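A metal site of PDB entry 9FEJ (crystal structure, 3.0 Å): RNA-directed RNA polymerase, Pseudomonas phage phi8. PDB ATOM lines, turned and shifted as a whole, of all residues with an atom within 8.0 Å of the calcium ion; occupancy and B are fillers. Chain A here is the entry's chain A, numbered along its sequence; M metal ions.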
ATOM      1  N   LEU A 321       1.112 -15.745 -11.934  1.00  0.00           N
ATOM      2  CA  LEU A 321       2.160 -14.798 -11.582  1.00  0.00           C
ATOM      3  C   LEU A 321       3.522 -15.448 -11.780  1.00  0.00           C
ATOM      4  O   LEU A 321       3.790 -16.518 -11.220  1.00  0.00           O
ATOM      5  CB  LEU A 321       2.001 -14.310 -10.140  1.00  0.00           C
ATOM      6  CG  LEU A 321       0.912 -13.245  -9.980  1.00  0.00           C
ATOM      7  CD1 LEU A 321       0.538 -13.038  -8.528  1.00  0.00           C
ATOM      8  CD2 LEU A 321       1.364 -11.934 -10.597  1.00  0.00           C
ATOM      9  N   TYR A 322       4.371 -14.809 -12.586  1.00  0.00           N
ATOM     10  CA  TYR A 322       5.673 -15.349 -12.941  1.00  0.00           C
ATOM     11  C   TYR A 322       6.755 -14.318 -12.684  1.00  0.00           C
ATOM     12  O   TYR A 322       6.559 -13.120 -12.912  1.00  0.00           O
ATOM     13  CB  TYR A 322       5.702 -15.779 -14.410  1.00  0.00           C
ATOM     14  CG  TYR A 322       5.112 -17.152 -14.658  1.00  0.00           C
ATOM     15  CD1 TYR A 322       3.745 -17.314 -14.836  1.00  0.00           C
ATOM     16  CD2 TYR A 322       5.922 -18.278 -14.706  1.00  0.00           C
ATOM     17  CE1 TYR A 322       3.201 -18.563 -15.055  1.00  0.00           C
ATOM     18  CE2 TYR A 322       5.392 -19.528 -14.926  1.00  0.00           C
ATOM     19  CZ  TYR A 322       4.023 -19.663 -15.092  1.00  0.00           C
ATOM     20  OH  TYR A 322       3.493 -20.913 -15.312  1.00  0.00           O
ATOM     21  N   ASP A 323       7.908 -14.791 -12.210  1.00  0.00           N
ATOM     22  CA  ASP A 323       9.072 -13.952 -11.982  1.00  0.00           C
ATOM     23  C   ASP A 323      10.228 -14.447 -12.846  1.00  0.00           C
ATOM     24  O   ASP A 323      10.390 -15.658 -13.043  1.00  0.00           O
ATOM     25  CB  ASP A 323       9.487 -13.958 -10.509  1.00  0.00           C
ATOM     26  CG  ASP A 323       8.469 -13.286  -9.612  1.00  0.00           C
ATOM     27  OD1 ASP A 323       7.434 -12.818 -10.127  1.00  0.00           O
ATOM     28  OD2 ASP A 323       8.693 -13.221  -8.386  1.00  0.00           O
ATOM     29  N   ALA A 324      11.018 -13.507 -13.364  1.00  0.00           N
ATOM     30  CA  ALA A 324      12.145 -13.840 -14.225  1.00  0.00           C
ATOM     31  C   ALA A 324      13.395 -14.061 -13.380  1.00  0.00           C
ATOM     32  O   ALA A 324      13.767 -13.207 -12.568  1.00  0.00           O
ATOM     33  CB  ALA A 324      12.392 -12.721 -15.245  1.00  0.00           C
ATOM     34  N   ASP A 445      10.763  -7.903 -14.696  1.00  0.00           N
ATOM     35  CA  ASP A 445      10.848  -9.313 -14.312  1.00  0.00           C
ATOM     36  C   ASP A 445       9.582  -9.814 -13.626  1.00  0.00           C
ATOM     37  O   ASP A 445       9.543 -10.976 -13.216  1.00  0.00           O
ATOM     38  CB  ASP A 445      12.046  -9.532 -13.388  1.00  0.00           C
ATOM     39  CG  ASP A 445      11.944  -8.754 -12.090  1.00  0.00           C
ATOM     40  OD1 ASP A 445      11.355  -7.659 -12.107  1.00  0.00           O
ATOM     41  OD2 ASP A 445      12.449  -9.244 -11.058  1.00  0.00           O
ATOM     42  N   ASP A 446       8.552  -8.987 -13.510  1.00  0.00           N
ATOM     43  CA  ASP A 446       7.285  -9.359 -12.888  1.00  0.00           C
ATOM     44  C   ASP A 446       6.190  -9.283 -13.934  1.00  0.00           C
ATOM     45  O   ASP A 446       5.897  -8.201 -14.463  1.00  0.00           O
ATOM     46  CB  ASP A 446       6.967  -8.431 -11.702  1.00  0.00           C
ATOM     47  CG  ASP A 446       6.921  -9.176 -10.382  1.00  0.00           C
ATOM     48  OD1 ASP A 446       6.223 -10.203 -10.309  1.00  0.00           O
ATOM     49  OD2 ASP A 446       7.604  -8.744  -9.430  1.00  0.00           O
ATOM     50  N   THR A 447       5.582 -10.435 -14.242  1.00  0.00           N
ATOM     51  CA  THR A 447       4.586 -10.530 -15.294  1.00  0.00           C
ATOM     52  C   THR A 447       3.396 -11.348 -14.808  1.00  0.00           C
ATOM     53  O   THR A 447       3.562 -12.371 -14.147  1.00  0.00           O
ATOM     54  CB  THR A 447       5.171 -11.176 -16.558  1.00  0.00           C
ATOM     55  OG1 THR A 447       6.319 -10.431 -16.985  1.00  0.00           O
ATOM     56  CG2 THR A 447       4.139 -11.188 -17.688  1.00  0.00           C
ATOM     57  N   MET A 448       2.195 -10.877 -15.127  1.00  0.00           N
ATOM     58  CA  MET A 448       0.952 -11.584 -14.820  1.00  0.00           C
ATOM     59  C   MET A 448       0.180 -11.830 -16.110  1.00  0.00           C
ATOM     60  O   MET A 448      -0.556 -10.943 -16.583  1.00  0.00           O
ATOM     61  CB  MET A 448       0.097 -10.793 -13.831  1.00  0.00           C
ATOM     62  CG  MET A 448      -1.237 -11.449 -13.489  1.00  0.00           C
ATOM     63  SD  MET A 448      -2.259 -10.463 -12.378  1.00  0.00           S
ATOM     64  CE  MET A 448      -2.540  -9.011 -13.381  1.00  0.00           C
ATOM     65  N   GLU A 473       9.738 -18.573 -13.906  1.00  0.00           N
ATOM     66  CA  GLU A 473       9.291 -19.518 -12.902  1.00  0.00           C
ATOM     67  C   GLU A 473       8.069 -18.966 -12.177  1.00  0.00           C
ATOM     68  O   GLU A 473       7.919 -17.745 -12.037  1.00  0.00           O
ATOM     69  CB  GLU A 473      10.404 -19.824 -11.887  1.00  0.00           C
ATOM     70  CG  GLU A 473      11.569 -20.606 -12.487  1.00  0.00           C
ATOM     71  CD  GLU A 473      12.790 -20.635 -11.575  1.00  0.00           C
ATOM     72  OE1 GLU A 473      13.081 -19.601 -10.942  1.00  0.00           O
ATOM     73  OE2 GLU A 473      13.431 -21.694 -11.480  1.00  0.00           O
ATOM     74  N   LYS A 474       7.202 -19.868 -11.727  1.00  0.00           N
ATOM     75  CA  LYS A 474       5.988 -19.464 -11.039  1.00  0.00           C
ATOM     76  C   LYS A 474       6.318 -18.772  -9.725  1.00  0.00           C
ATOM     77  O   LYS A 474       7.155 -19.235  -8.947  1.00  0.00           O
ATOM     78  CB  LYS A 474       5.104 -20.688 -10.766  1.00  0.00           C
ATOM     79  CG  LYS A 474       4.442 -21.278 -11.996  1.00  0.00           C
ATOM     80  CD  LYS A 474       3.447 -22.368 -11.608  1.00  0.00           C
ATOM     81  CE  LYS A 474       2.745 -22.946 -12.816  1.00  0.00           C
ATOM     82  NZ  LYS A 474       1.754 -23.996 -12.442  1.00  0.00           N
ATOM     83  N   ASP A 475       5.663 -17.642  -9.482  1.00  0.00           N
ATOM     84  CA  ASP A 475       5.830 -16.915  -8.227  1.00  0.00           C
ATOM     85  C   ASP A 475       5.064 -17.656  -7.141  1.00  0.00           C
ATOM     86  O   ASP A 475       3.831 -17.692  -7.152  1.00  0.00           O
ATOM     87  CB  ASP A 475       5.336 -15.469  -8.370  1.00  0.00           C
ATOM     88  CG  ASP A 475       5.781 -14.588  -7.214  1.00  0.00           C
ATOM     89  OD1 ASP A 475       6.182 -15.119  -6.159  1.00  0.00           O
ATOM     90  OD2 ASP A 475       5.716 -13.354  -7.362  1.00  0.00           O
ATOM     91  N   THR A 476       5.802 -18.239  -6.198  1.00  0.00           N
ATOM     92  CA  THR A 476       5.158 -18.938  -5.086  1.00  0.00           C
ATOM     93  C   THR A 476       4.517 -17.984  -4.099  1.00  0.00           C
ATOM     94  O   THR A 476       3.596 -18.374  -3.379  1.00  0.00           O
ATOM     95  CB  THR A 476       6.179 -19.831  -4.365  1.00  0.00           C
ATOM     96  OG1 THR A 476       7.341 -19.046  -4.034  1.00  0.00           O
ATOM     97  CG2 THR A 476       6.584 -20.996  -5.248  1.00  0.00           C
ATOM     98  N   GLY A 477       4.988 -16.731  -4.043  1.00  0.00           N
ATOM     99  CA  GLY A 477       4.409 -15.766  -3.118  1.00  0.00           C
ATOM    100  C   GLY A 477       3.135 -15.116  -3.596  1.00  0.00           C
ATOM    101  O   GLY A 477       2.390 -14.569  -2.781  1.00  0.00           O
ATOM    102  N   LYS A 478       2.866 -15.161  -4.908  1.00  0.00           N
ATOM    103  CA  LYS A 478       1.660 -14.559  -5.483  1.00  0.00           C
ATOM    104  C   LYS A 478       1.583 -13.063  -5.176  1.00  0.00           C
ATOM    105  O   LYS A 478       0.562 -12.547  -4.736  1.00  0.00           O
ATOM    106  CB  LYS A 478       0.396 -15.282  -5.009  1.00  0.00           C
ATOM    107  CG  LYS A 478       0.127 -16.607  -5.717  1.00  0.00           C
ATOM    108  CD  LYS A 478      -0.407 -16.391  -7.121  1.00  0.00           C
ATOM    109  CE  LYS A 478      -0.765 -17.713  -7.779  1.00  0.00           C
ATOM    110  NZ  LYS A 478      -1.391 -17.519  -9.124  1.00  0.00           N
ATOM    111  N   LYS A 479       2.694 -12.370  -5.413  1.00  0.00           N
ATOM    112  CA  LYS A 479       2.759 -10.918  -5.276  1.00  0.00           C
ATOM    113  C   LYS A 479       3.066 -10.293  -6.625  1.00  0.00           C
ATOM    114  O   LYS A 479       3.857 -10.836  -7.415  1.00  0.00           O
ATOM    115  CB  LYS A 479       3.815 -10.501  -4.252  1.00  0.00           C
ATOM    116  CG  LYS A 479       3.343 -10.564  -2.807  1.00  0.00           C
ATOM    117  CD  LYS A 479       4.251  -9.754  -1.887  1.00  0.00           C
ATOM    118  CE  LYS A 479       5.666 -10.309  -1.878  1.00  0.00           C
ATOM    119  NZ  LYS A 479       6.553  -9.543  -0.963  1.00  0.00           N
ATOM    120  N   PHE A 480       2.370  -9.218  -6.953  1.00  0.00           N
ATOM    121  CA  PHE A 480       2.638  -8.506  -8.190  1.00  0.00           C
ATOM    122  C   PHE A 480       3.108  -7.167  -7.728  1.00  0.00           C
ATOM    123  O   PHE A 480       2.396  -6.479  -6.995  1.00  0.00           O
ATOM    124  CB  PHE A 480       1.389  -8.379  -9.047  1.00  0.00           C
ATOM    125  CG  PHE A 480       1.663  -7.841 -10.417  1.00  0.00           C
ATOM    126  CD1 PHE A 480       2.694  -8.351 -11.189  1.00  0.00           C
ATOM    127  CD2 PHE A 480       0.892  -6.811 -10.944  1.00  0.00           C
ATOM    128  CE1 PHE A 480       2.946  -7.858 -12.457  1.00  0.00           C
ATOM    129  CE2 PHE A 480       1.144  -6.318 -12.212  1.00  0.00           C
ATOM    130  CZ  PHE A 480       2.167  -6.845 -12.968  1.00  0.00           C
ATOM    131  N   ILE A 481       4.313  -6.776  -8.118  1.00  0.00           N
ATOM    132  CA  ILE A 481       4.872  -5.547  -7.597  1.00  0.00           C
ATOM    133  C   ILE A 481       4.927  -5.756  -6.105  1.00  0.00           C
ATOM    134  O   ILE A 481       5.666  -6.612  -5.632  1.00  0.00           O
ATOM    135  CB  ILE A 481       4.029  -4.315  -7.973  1.00  0.00           C
ATOM    136  CG1 ILE A 481       3.881  -4.215  -9.483  1.00  0.00           C
ATOM    137  CG2 ILE A 481       4.681  -3.044  -7.433  1.00  0.00           C
ATOM    138  CD1 ILE A 481       5.207  -4.125 -10.208  1.00  0.00           C
ATOM    139  N   GLY A 482       4.155  -4.993  -5.348  1.00  0.00           N
ATOM    140  CA  GLY A 482       4.109  -5.181  -3.916  1.00  0.00           C
ATOM    141  C   GLY A 482       2.683  -5.416  -3.492  1.00  0.00           C
ATOM    142  O   GLY A 482       2.286  -5.001  -2.404  1.00  0.00           O
ATOM    143  N   ARG A 483       1.907  -6.060  -4.343  1.00  0.00           N
ATOM    144  CA  ARG A 483       0.496  -6.235  -4.047  1.00  0.00           C
ATOM    145  C   ARG A 483       0.098  -7.672  -3.805  1.00  0.00           C
ATOM    146  O   ARG A 483       0.223  -8.515  -4.693  1.00  0.00           O
ATOM    147  CB  ARG A 483      -0.355  -5.659  -5.178  1.00  0.00           C
ATOM    148  CG  ARG A 483       0.168  -4.338  -5.721  1.00  0.00           C
ATOM    149  CD  ARG A 483       0.043  -3.232  -4.678  1.00  0.00           C
ATOM    150  NE  ARG A 483      -1.223  -3.299  -3.955  1.00  0.00           N
ATOM    151  CZ  ARG A 483      -1.581  -2.471  -2.987  1.00  0.00           C
ATOM    152  NH1 ARG A 483      -0.762  -1.488  -2.623  1.00  0.00           N
ATOM    153  NH2 ARG A 483      -2.748  -2.607  -2.389  1.00  0.00           N
HETATM  154 CA    CA M   1       5.785 -11.445  -8.499  1.00  0.00          CA
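The backbone carbonyl oxygen of Leu 321 lies within hydrogen-bond range of the backbone NH of Asp 475, 2.8 Å away.
The backbone NH (N) of Gly 477 is in hydrogen-bond range of the side-chain carboxylate (OD1) of Asp 475 (2.9 Å).
The backbone carbonyl oxygen (O) of Glu 473 is in hydrogen-bond range of the backbone NH (N) of Asp 323 (3.0 Å).
Four residues have an atom within 4 Å of the calcium ion: Asp 323, Asp 446, Asp 475 and Lys 479.
The calcium ion is bound by OD2 of Asp 475 (2.2 Å), OD1 of Asp 446 (2.2 Å), O of Lys 479 (2.3 Å) and OD1 of Asp 323 (2.7 Å).
The calcium ion has four donor atoms within binding distance.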
